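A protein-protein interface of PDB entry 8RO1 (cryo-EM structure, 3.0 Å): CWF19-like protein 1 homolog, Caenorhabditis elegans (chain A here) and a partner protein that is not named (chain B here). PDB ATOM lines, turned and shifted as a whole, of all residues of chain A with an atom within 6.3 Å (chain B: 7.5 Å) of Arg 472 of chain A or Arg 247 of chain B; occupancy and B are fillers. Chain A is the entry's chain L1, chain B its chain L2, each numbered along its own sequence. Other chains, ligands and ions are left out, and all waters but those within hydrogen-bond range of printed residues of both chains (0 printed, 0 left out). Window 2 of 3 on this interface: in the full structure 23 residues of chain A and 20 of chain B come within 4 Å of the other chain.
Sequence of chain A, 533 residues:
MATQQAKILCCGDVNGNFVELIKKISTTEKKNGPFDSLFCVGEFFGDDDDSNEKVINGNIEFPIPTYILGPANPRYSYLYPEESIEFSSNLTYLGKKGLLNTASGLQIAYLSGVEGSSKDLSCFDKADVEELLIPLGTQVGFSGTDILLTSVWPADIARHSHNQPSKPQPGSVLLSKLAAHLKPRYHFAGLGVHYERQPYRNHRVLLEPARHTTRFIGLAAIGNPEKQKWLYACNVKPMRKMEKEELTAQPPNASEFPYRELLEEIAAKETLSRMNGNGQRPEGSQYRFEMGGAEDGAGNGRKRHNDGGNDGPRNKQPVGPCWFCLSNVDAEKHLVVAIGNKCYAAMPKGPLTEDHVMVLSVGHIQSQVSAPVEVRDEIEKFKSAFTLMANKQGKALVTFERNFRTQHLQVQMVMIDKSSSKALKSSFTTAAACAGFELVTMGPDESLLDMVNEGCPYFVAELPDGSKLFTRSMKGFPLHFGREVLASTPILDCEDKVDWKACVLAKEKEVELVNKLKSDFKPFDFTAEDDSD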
ATOM      1  N   GLU A 438       3.079  15.063  -0.020  1.00  0.00           N
ATOM      2  CA  GLU A 438       2.380  13.979   0.659  1.00  0.00           C
ATOM      3  C   GLU A 438       1.298  14.558   1.561  1.00  0.00           C
ATOM      4  O   GLU A 438       1.580  15.422   2.399  1.00  0.00           O
ATOM      5  CB  GLU A 438       3.362  13.148   1.486  1.00  0.00           C
ATOM      6  CG  GLU A 438       2.755  11.914   2.125  1.00  0.00           C
ATOM      7  CD  GLU A 438       3.806  10.885   2.493  1.00  0.00           C
ATOM      8  OE1 GLU A 438       4.889  11.288   2.968  1.00  0.00           O
ATOM      9  OE2 GLU A 438       3.563   9.679   2.286  1.00  0.00           O
ATOM     10  N   MET A 451      -1.143  19.406  14.945  1.00  0.00           N
ATOM     11  CA  MET A 451       0.035  19.084  14.141  1.00  0.00           C
ATOM     12  C   MET A 451       1.018  20.238  14.021  1.00  0.00           C
ATOM     13  O   MET A 451       2.227  19.995  13.925  1.00  0.00           O
ATOM     14  CB  MET A 451      -0.384  18.626  12.744  1.00  0.00           C
ATOM     15  CG  MET A 451      -0.762  17.160  12.652  1.00  0.00           C
ATOM     16  SD  MET A 451       0.566  15.980  13.026  1.00  0.00           S
ATOM     17  CE  MET A 451       1.739  16.318  11.713  1.00  0.00           C
ATOM     18  N   VAL A 452       0.542  21.486  14.013  1.00  0.00           N
ATOM     19  CA  VAL A 452       1.406  22.641  13.799  1.00  0.00           C
ATOM     20  C   VAL A 452       0.974  23.790  14.699  1.00  0.00           C
ATOM     21  O   VAL A 452      -0.173  23.878  15.139  1.00  0.00           O
ATOM     22  CB  VAL A 452       1.422  23.106  12.319  1.00  0.00           C
ATOM     23  CG1 VAL A 452       2.087  22.061  11.431  1.00  0.00           C
ATOM     24  CG2 VAL A 452       0.006  23.416  11.805  1.00  0.00           C
ATOM     25  N   ASN A 453       1.935  24.666  14.966  1.00  0.00           N
ATOM     26  CA  ASN A 453       1.766  25.860  15.774  1.00  0.00           C
ATOM     27  C   ASN A 453       1.421  27.064  14.898  1.00  0.00           C
ATOM     28  O   ASN A 453       1.441  26.997  13.666  1.00  0.00           O
ATOM     29  CB  ASN A 453       3.038  26.107  16.580  1.00  0.00           C
ATOM     30  CG  ASN A 453       3.208  25.105  17.707  1.00  0.00           C
ATOM     31  OD1 ASN A 453       2.670  25.282  18.799  1.00  0.00           O
ATOM     32  ND2 ASN A 453       3.918  24.017  17.428  1.00  0.00           N
ATOM     33  N   CYS A 456       2.526  28.890  10.961  1.00  0.00           N
ATOM     34  CA  CYS A 456       2.904  27.958   9.909  1.00  0.00           C
ATOM     35  C   CYS A 456       1.824  27.935   8.828  1.00  0.00           C
ATOM     36  O   CYS A 456       0.651  27.723   9.149  1.00  0.00           O
ATOM     37  CB  CYS A 456       3.073  26.560  10.486  1.00  0.00           C
ATOM     38  SG  CYS A 456       3.663  25.323   9.305  1.00  0.00           S
ATOM     39  N   PRO A 457       2.161  28.138   7.548  1.00  0.00           N
ATOM     40  CA  PRO A 457       1.151  27.898   6.511  1.00  0.00           C
ATOM     41  C   PRO A 457       0.891  26.408   6.385  1.00  0.00           C
ATOM     42  O   PRO A 457       1.810  25.590   6.476  1.00  0.00           O
ATOM     43  CB  PRO A 457       1.775  28.482   5.237  1.00  0.00           C
ATOM     44  CG  PRO A 457       2.912  29.302   5.670  1.00  0.00           C
ATOM     45  CD  PRO A 457       3.361  28.796   6.992  1.00  0.00           C
ATOM     46  N   TYR A 458      -0.374  26.058   6.179  1.00  0.00           N
ATOM     47  CA  TYR A 458      -0.758  24.658   6.110  1.00  0.00           C
ATOM     48  C   TYR A 458      -2.050  24.530   5.322  1.00  0.00           C
ATOM     49  O   TYR A 458      -2.838  25.475   5.238  1.00  0.00           O
ATOM     50  CB  TYR A 458      -0.925  24.049   7.513  1.00  0.00           C
ATOM     51  CG  TYR A 458      -2.079  24.609   8.333  1.00  0.00           C
ATOM     52  CD1 TYR A 458      -3.358  24.056   8.256  1.00  0.00           C
ATOM     53  CD2 TYR A 458      -1.891  25.687   9.182  1.00  0.00           C
ATOM     54  CE1 TYR A 458      -4.406  24.568   8.989  1.00  0.00           C
ATOM     55  CE2 TYR A 458      -2.935  26.203   9.927  1.00  0.00           C
ATOM     56  CZ  TYR A 458      -4.190  25.639   9.825  1.00  0.00           C
ATOM     57  OH  TYR A 458      -5.233  26.143  10.568  1.00  0.00           O
ATOM     58  N   PHE A 459      -2.241  23.350   4.739  1.00  0.00           N
ATOM     59  CA  PHE A 459      -3.498  22.959   4.124  1.00  0.00           C
ATOM     60  C   PHE A 459      -3.983  21.695   4.815  1.00  0.00           C
ATOM     61  O   PHE A 459      -3.188  20.799   5.120  1.00  0.00           O
ATOM     62  CB  PHE A 459      -3.339  22.721   2.619  1.00  0.00           C
ATOM     63  CG  PHE A 459      -4.600  22.268   1.940  1.00  0.00           C
ATOM     64  CD1 PHE A 459      -5.534  23.193   1.508  1.00  0.00           C
ATOM     65  CD2 PHE A 459      -4.832  20.923   1.698  1.00  0.00           C
ATOM     66  CE1 PHE A 459      -6.692  22.784   0.876  1.00  0.00           C
ATOM     67  CE2 PHE A 459      -5.986  20.509   1.064  1.00  0.00           C
ATOM     68  CZ  PHE A 459      -6.919  21.441   0.654  1.00  0.00           C
ATOM     69  N   PHE A 470      -3.745  16.101   5.800  1.00  0.00           N
ATOM     70  CA  PHE A 470      -2.966  17.270   6.190  1.00  0.00           C
ATOM     71  C   PHE A 470      -1.606  17.215   5.509  1.00  0.00           C
ATOM     72  O   PHE A 470      -1.059  16.134   5.274  1.00  0.00           O
ATOM     73  CB  PHE A 470      -2.814  17.319   7.722  1.00  0.00           C
ATOM     74  CG  PHE A 470      -1.937  18.433   8.223  1.00  0.00           C
ATOM     75  CD1 PHE A 470      -2.445  19.709   8.386  1.00  0.00           C
ATOM     76  CD2 PHE A 470      -0.613  18.197   8.554  1.00  0.00           C
ATOM     77  CE1 PHE A 470      -1.647  20.730   8.858  1.00  0.00           C
ATOM     78  CE2 PHE A 470       0.191  19.216   9.023  1.00  0.00           C
ATOM     79  CZ  PHE A 470      -0.325  20.486   9.171  1.00  0.00           C
ATOM     80  N   THR A 471      -1.064  18.391   5.190  1.00  0.00           N
ATOM     81  CA  THR A 471       0.268  18.488   4.610  1.00  0.00           C
ATOM     82  C   THR A 471       0.909  19.806   5.014  1.00  0.00           C
ATOM     83  O   THR A 471       0.228  20.826   5.159  1.00  0.00           O
ATOM     84  CB  THR A 471       0.227  18.373   3.076  1.00  0.00           C
ATOM     85  OG1 THR A 471       1.563  18.337   2.558  1.00  0.00           O
ATOM     86  CG2 THR A 471      -0.555  19.541   2.433  1.00  0.00           C
ATOM     87  N   ARG A 472       2.231  19.770   5.187  1.00  0.00           N
ATOM     88  CA  ARG A 472       3.025  20.948   5.503  1.00  0.00           C
ATOM     89  C   ARG A 472       3.785  21.508   4.307  1.00  0.00           C
ATOM     90  O   ARG A 472       4.340  22.606   4.410  1.00  0.00           O
ATOM     91  CB  ARG A 472       4.032  20.643   6.608  1.00  0.00           C
ATOM     92  CG  ARG A 472       3.409  20.391   7.975  1.00  0.00           C
ATOM     93  CD  ARG A 472       4.446  20.284   9.101  1.00  0.00           C
ATOM     94  NE  ARG A 472       5.174  21.532   9.333  1.00  0.00           N
ATOM     95  CZ  ARG A 472       6.271  21.937   8.700  1.00  0.00           C
ATOM     96  NH1 ARG A 472       6.680  23.192   8.861  1.00  0.00           N
ATOM     97  NH2 ARG A 472       6.995  21.116   7.955  1.00  0.00           N
ATOM     98  N   SER A 473       3.846  20.783   3.192  1.00  0.00           N
ATOM     99  CA  SER A 473       4.619  21.212   2.030  1.00  0.00           C
ATOM    100  C   SER A 473       3.807  22.260   1.286  1.00  0.00           C
ATOM    101  O   SER A 473       2.969  21.944   0.438  1.00  0.00           O
ATOM    102  CB  SER A 473       4.956  20.026   1.138  1.00  0.00           C
ATOM    103  OG  SER A 473       5.764  19.085   1.822  1.00  0.00           O
ATOM    104  N   MET A 474       4.074  23.528   1.609  1.00  0.00           N
ATOM    105  CA  MET A 474       3.325  24.658   1.078  1.00  0.00           C
ATOM    106  C   MET A 474       4.094  25.468   0.044  1.00  0.00           C
ATOM    107  O   MET A 474       3.514  26.378  -0.556  1.00  0.00           O
ATOM    108  CB  MET A 474       2.892  25.588   2.217  1.00  0.00           C
ATOM    109  CG  MET A 474       2.054  24.918   3.303  1.00  0.00           C
ATOM    110  SD  MET A 474       0.603  24.009   2.730  1.00  0.00           S
ATOM    111  CE  MET A 474      -0.476  25.369   2.300  1.00  0.00           C
ATOM    112  N   LYS A 475       5.370  25.167  -0.185  1.00  0.00           N
ATOM    113  CA  LYS A 475       6.135  25.849  -1.220  1.00  0.00           C
ATOM    114  C   LYS A 475       5.610  25.437  -2.590  1.00  0.00           C
ATOM    115  O   LYS A 475       5.698  24.263  -2.966  1.00  0.00           O
ATOM    116  CB  LYS A 475       7.616  25.507  -1.082  1.00  0.00           C
ATOM    117  CG  LYS A 475       8.539  26.366  -1.927  1.00  0.00           C
ATOM    118  CD  LYS A 475       9.995  26.000  -1.688  1.00  0.00           C
ATOM    119  CE  LYS A 475      10.930  26.826  -2.555  1.00  0.00           C
ATOM    120  NZ  LYS A 475      12.360  26.474  -2.331  1.00  0.00           N
ATOM    121  N   ARG B 234      16.912  31.746  13.265  1.00  0.00           N
ATOM    122  CA  ARG B 234      16.625  30.632  12.364  1.00  0.00           C
ATOM    123  C   ARG B 234      16.786  29.276  13.049  1.00  0.00           C
ATOM    124  O   ARG B 234      15.990  28.360  12.812  1.00  0.00           O
ATOM    125  CB  ARG B 234      17.516  30.714  11.122  1.00  0.00           C
ATOM    126  CG  ARG B 234      17.138  29.707  10.046  1.00  0.00           C
ATOM    127  CD  ARG B 234      17.944  29.866   8.774  1.00  0.00           C
ATOM    128  NE  ARG B 234      17.518  28.883   7.782  1.00  0.00           N
ATOM    129  CZ  ARG B 234      17.979  28.788   6.540  1.00  0.00           C
ATOM    130  NH1 ARG B 234      17.472  27.859   5.734  1.00  0.00           N
ATOM    131  NH2 ARG B 234      18.923  29.595   6.078  1.00  0.00           N
ATOM    132  N   ASP B 237      13.575  28.668  14.799  1.00  0.00           N
ATOM    133  CA  ASP B 237      12.391  28.533  13.962  1.00  0.00           C
ATOM    134  C   ASP B 237      12.424  27.268  13.118  1.00  0.00           C
ATOM    135  O   ASP B 237      11.381  26.644  12.899  1.00  0.00           O
ATOM    136  CB  ASP B 237      12.264  29.758  13.058  1.00  0.00           C
ATOM    137  CG  ASP B 237      11.814  31.004  13.807  1.00  0.00           C
ATOM    138  OD1 ASP B 237      11.352  30.891  14.963  1.00  0.00           O
ATOM    139  OD2 ASP B 237      11.930  32.108  13.235  1.00  0.00           O
ATOM    140  N   ASP B 238      13.596  26.875  12.640  1.00  0.00           N
ATOM    141  CA  ASP B 238      13.755  25.614  11.929  1.00  0.00           C
ATOM    142  C   ASP B 238      13.965  24.411  12.843  1.00  0.00           C
ATOM    143  O   ASP B 238      14.116  23.296  12.334  1.00  0.00           O
ATOM    144  CB  ASP B 238      14.935  25.730  10.962  1.00  0.00           C
ATOM    145  CG  ASP B 238      14.585  26.488   9.685  1.00  0.00           C
ATOM    146  OD1 ASP B 238      13.388  26.695   9.394  1.00  0.00           O
ATOM    147  OD2 ASP B 238      15.523  26.877   8.959  1.00  0.00           O
ATOM    148  N   CYS B 239      13.962  24.585  14.161  1.00  0.00           N
ATOM    149  CA  CYS B 239      14.022  23.446  15.069  1.00  0.00           C
ATOM    150  C   CYS B 239      12.707  22.682  15.056  1.00  0.00           C
ATOM    151  O   CYS B 239      11.663  23.220  15.432  1.00  0.00           O
ATOM    152  CB  CYS B 239      14.348  23.896  16.484  1.00  0.00           C
ATOM    153  SG  CYS B 239      14.430  22.522  17.607  1.00  0.00           S
ATOM    154  N   SER B 240      12.761  21.430  14.617  1.00  0.00           N
ATOM    155  CA  SER B 240      11.601  20.551  14.608  1.00  0.00           C
ATOM    156  C   SER B 240      11.357  19.860  15.944  1.00  0.00           C
ATOM    157  O   SER B 240      10.318  19.213  16.094  1.00  0.00           O
ATOM    158  CB  SER B 240      11.755  19.497  13.519  1.00  0.00           C
ATOM    159  OG  SER B 240      12.911  18.714  13.740  1.00  0.00           O
ATOM    160  N   ARG B 241      12.288  19.949  16.897  1.00  0.00           N
ATOM    161  CA  ARG B 241      12.224  19.191  18.143  1.00  0.00           C
ATOM    162  C   ARG B 241      11.422  19.873  19.246  1.00  0.00           C
ATOM    163  O   ARG B 241      10.817  19.178  20.067  1.00  0.00           O
ATOM    164  CB  ARG B 241      13.641  18.937  18.658  1.00  0.00           C
ATOM    165  CG  ARG B 241      14.480  17.998  17.809  1.00  0.00           C
ATOM    166  CD  ARG B 241      14.079  16.564  18.001  1.00  0.00           C
ATOM    167  NE  ARG B 241      14.745  15.695  17.040  1.00  0.00           N
ATOM    168  CZ  ARG B 241      14.264  15.339  15.856  1.00  0.00           C
ATOM    169  NH1 ARG B 241      15.009  14.586  15.058  1.00  0.00           N
ATOM    170  NH2 ARG B 241      13.055  15.695  15.452  1.00  0.00           N
ATOM    171  N   CYS B 242      11.388  21.201  19.291  1.00  0.00           N
ATOM    172  CA  CYS B 242      10.584  21.890  20.294  1.00  0.00           C
ATOM    173  C   CYS B 242       9.108  21.613  20.070  1.00  0.00           C
ATOM    174  O   CYS B 242       8.652  21.477  18.934  1.00  0.00           O
ATOM    175  CB  CYS B 242      10.826  23.398  20.275  1.00  0.00           C
ATOM    176  SG  CYS B 242      12.523  23.924  20.453  1.00  0.00           S
ATOM    177  N   ASP B 244       6.828  23.686  20.587  1.00  0.00           N
ATOM    178  CA  ASP B 244       6.344  24.871  19.892  1.00  0.00           C
ATOM    179  C   ASP B 244       6.720  24.912  18.417  1.00  0.00           C
ATOM    180  O   ASP B 244       6.433  25.916  17.757  1.00  0.00           O
ATOM    181  CB  ASP B 244       6.881  26.123  20.578  1.00  0.00           C
ATOM    182  CG  ASP B 244       6.503  26.187  22.039  1.00  0.00           C
ATOM    183  OD1 ASP B 244       5.290  26.184  22.335  1.00  0.00           O
ATOM    184  OD2 ASP B 244       7.413  26.243  22.892  1.00  0.00           O
ATOM    185  N   SER B 245       7.348  23.874  17.875  1.00  0.00           N
ATOM    186  CA  SER B 245       7.825  23.937  16.504  1.00  0.00           C
ATOM    187  C   SER B 245       6.672  23.910  15.510  1.00  0.00           C
ATOM    188  O   SER B 245       5.666  23.223  15.706  1.00  0.00           O
ATOM    189  CB  SER B 245       8.776  22.785  16.207  1.00  0.00           C
ATOM    190  OG  SER B 245       9.272  22.908  14.888  1.00  0.00           O
ATOM    191  N   SER B 246       6.850  24.656  14.423  1.00  0.00           N
ATOM    192  CA  SER B 246       6.014  24.506  13.240  1.00  0.00           C
ATOM    193  C   SER B 246       6.341  23.246  12.452  1.00  0.00           C
ATOM    194  O   SER B 246       5.507  22.798  11.657  1.00  0.00           O
ATOM    195  CB  SER B 246       6.186  25.725  12.336  1.00  0.00           C
ATOM    196  OG  SER B 246       7.544  25.894  11.969  1.00  0.00           O
ATOM    197  N   ARG B 247       7.518  22.660  12.664  1.00  0.00           N
ATOM    198  CA  ARG B 247       7.958  21.471  11.951  1.00  0.00           C
ATOM    199  C   ARG B 247       7.766  20.204  12.771  1.00  0.00           C
ATOM    200  O   ARG B 247       8.333  19.161  12.429  1.00  0.00           O
ATOM    201  CB  ARG B 247       9.424  21.624  11.548  1.00  0.00           C
ATOM    202  CG  ARG B 247       9.666  22.777  10.600  1.00  0.00           C
ATOM    203  CD  ARG B 247      11.089  22.798  10.108  1.00  0.00           C
ATOM    204  NE  ARG B 247      11.313  23.905   9.186  1.00  0.00           N
ATOM    205  CZ  ARG B 247      11.136  23.863   7.868  1.00  0.00           C
ATOM    206  NH1 ARG B 247      11.414  24.942   7.145  1.00  0.00           N
ATOM    207  NH2 ARG B 247      10.686  22.778   7.254  1.00  0.00           N
ATOM    208  N   LEU B 248       6.985  20.280  13.847  1.00  0.00           N
ATOM    209  CA  LEU B 248       6.841  19.181  14.786  1.00  0.00           C
ATOM    210  C   LEU B 248       6.202  17.987  14.094  1.00  0.00           C
ATOM    211  O   LEU B 248       5.368  18.136  13.196  1.00  0.00           O
ATOM    212  CB  LEU B 248       6.003  19.615  15.984  1.00  0.00           C
ATOM    213  CG  LEU B 248       5.819  18.616  17.125  1.00  0.00           C
ATOM    214  CD1 LEU B 248       7.130  18.257  17.797  1.00  0.00           C
ATOM    215  CD2 LEU B 248       4.850  19.208  18.132  1.00  0.00           C
ATOM    216  N   LYS B 249       6.611  16.791  14.512  1.00  0.00           N
ATOM    217  CA  LYS B 249       5.941  15.547  14.139  1.00  0.00           C
ATOM    218  C   LYS B 249       5.425  14.902  15.415  1.00  0.00           C
ATOM    219  O   LYS B 249       6.048  14.013  15.995  1.00  0.00           O
ATOM    220  CB  LYS B 249       6.889  14.640  13.379  1.00  0.00           C
ATOM    221  CG  LYS B 249       7.208  15.161  11.988  1.00  0.00           C
ATOM    222  CD  LYS B 249       8.102  14.214  11.212  1.00  0.00           C
ATOM    223  CE  LYS B 249       8.505  14.810   9.871  1.00  0.00           C
ATOM    224  NZ  LYS B 249       9.432  13.915   9.128  1.00  0.00           N
ATOM    225  N   LYS B 250       4.262  15.390  15.849  1.00  0.00           N
ATOM    226  CA  LYS B 250       3.732  15.097  17.172  1.00  0.00           C
ATOM    227  C   LYS B 250       3.263  13.659  17.310  1.00  0.00           C
ATOM    228  O   LYS B 250       3.209  13.144  18.429  1.00  0.00           O
ATOM    229  CB  LYS B 250       2.562  16.032  17.480  1.00  0.00           C
ATOM    230  CG  LYS B 250       2.469  16.488  18.924  1.00  0.00           C
ATOM    231  CD  LYS B 250       1.548  17.693  19.071  1.00  0.00           C
ATOM    232  CE  LYS B 250       1.677  18.330  20.441  1.00  0.00           C
ATOM    233  NZ  LYS B 250       0.905  19.596  20.529  1.00  0.00           N
ATOM    234  N   ASN B 252       4.971  11.208  16.535  1.00  0.00           N
ATOM    235  CA  ASN B 252       6.120  10.449  17.008  1.00  0.00           C
ATOM    236  C   ASN B 252       6.025  10.134  18.495  1.00  0.00           C
ATOM    237  O   ASN B 252       6.562   9.119  18.946  1.00  0.00           O
ATOM    238  CB  ASN B 252       7.396  11.226  16.711  1.00  0.00           C
ATOM    239  CG  ASN B 252       7.589  11.461  15.242  1.00  0.00           C
ATOM    240  OD1 ASN B 252       6.820  10.966  14.418  1.00  0.00           O
ATOM    241  ND2 ASN B 252       8.617  12.227  14.893  1.00  0.00           N
ATOM    242  N   GLU B 266      12.282   9.368  13.439  1.00  0.00           N
ATOM    243  CA  GLU B 266      11.630   9.764  12.199  1.00  0.00           C
ATOM    244  C   GLU B 266      11.981   8.895  10.999  1.00  0.00           C
ATOM    245  O   GLU B 266      11.500   9.189   9.900  1.00  0.00           O
ATOM    246  CB  GLU B 266      12.019  11.204  11.873  1.00  0.00           C
ATOM    247  CG  GLU B 266      11.743  12.204  12.970  1.00  0.00           C
ATOM    248  CD  GLU B 266      12.124  13.612  12.566  1.00  0.00           C
ATOM    249  OE1 GLU B 266      11.687  14.059  11.483  1.00  0.00           O
ATOM    250  OE2 GLU B 266      12.870  14.268  13.321  1.00  0.00           O
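The side-chain amide nitrogen (ND2) of Asn 453 of chain A lies close to the backbone carbonyl oxygen (O) of Asp 244 of chain B (3.2 Å). ND2 of Asn 453 of chain A lies within hydrogen-bond range of O of Ser 245 of chain B, at 2.6 Å. O of Ser 246 of chain B lies within hydrogen-bond range of NE of Arg 472 of chain A, at 2.7 Å.
The guanidinium group of Arg 472 of chain A sits at hydrogen-bond distance from the side-chain sulfur of Cys 456 of chain A, 3.7 Å away. The guanidinium group (NH1) of Arg 247 of chain B is in salt-bridge range of the side-chain carboxylate (OD1) of Asp 238 of chain B, 3.5 Å away. The backbone carbonyl oxygen of Cys 239 of chain B sits at hydrogen-bond distance from the side-chain hydroxyl of Ser 245 of chain B, 2.5 Å away. The backbone NH of Arg 247 of chain B sits at hydrogen-bond distance from the side-chain hydroxyl of Ser 245 of chain B (2.8 Å).
Among the printed residues, merely in contact across the chains: Arg 472 of chain A with Arg 247 of chain B, Val 452 of chain A with Ser 246 of chain B, Cys 456 of chain A with Ser 246 of chain B and Met 451 of chain A with Leu 248 of chain B.
Printed residues of chain B within 4 Å of Met 451 of chain A: Leu 248 (3.7 Å). Printed residues of chain B within 4 Å of Cys 456 of chain A: Ser 246. Pro 457 of chain A touches none of the printed residues of chain B. Arg 472 of chain A touches two residues of chain B. Printed residues of chain A within 4 Å of Asp 244 of chain B: Asn 453. Printed residues of chain A within 4 Å of Ser 245 of chain B: Asn 453 (2.6 Å). Of the printed residues of chain A, Arg 247 of chain B touches Arg 472 (3.5 Å). Lys 249 of chain B touches none of the printed residues of chain A. The nearest residue of chain A that does not touch Arg 247 of chain B is Val 452 of chain A (5.6 Å). The nearest printed residue of chain A that does not touch Ser 245 of chain B is Val 452 of chain A (4.7 Å).
Of the 16 printed residues of chain B, 5 touch a printed residue of chain A. Of the 14 printed residues of chain A, 5 touch a printed residue of chain B. Hydrophobic or aromatic side chains of chain A within 4 Å of the printed part of chain B: Val 452. Along chain A the printed residues that touch a printed residue of chain B span positions 451 to 472. Among the printed residues, no Asp or Glu carboxylate lies within 4 Å of a Lys or Arg side-chain nitrogen of the other chain.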
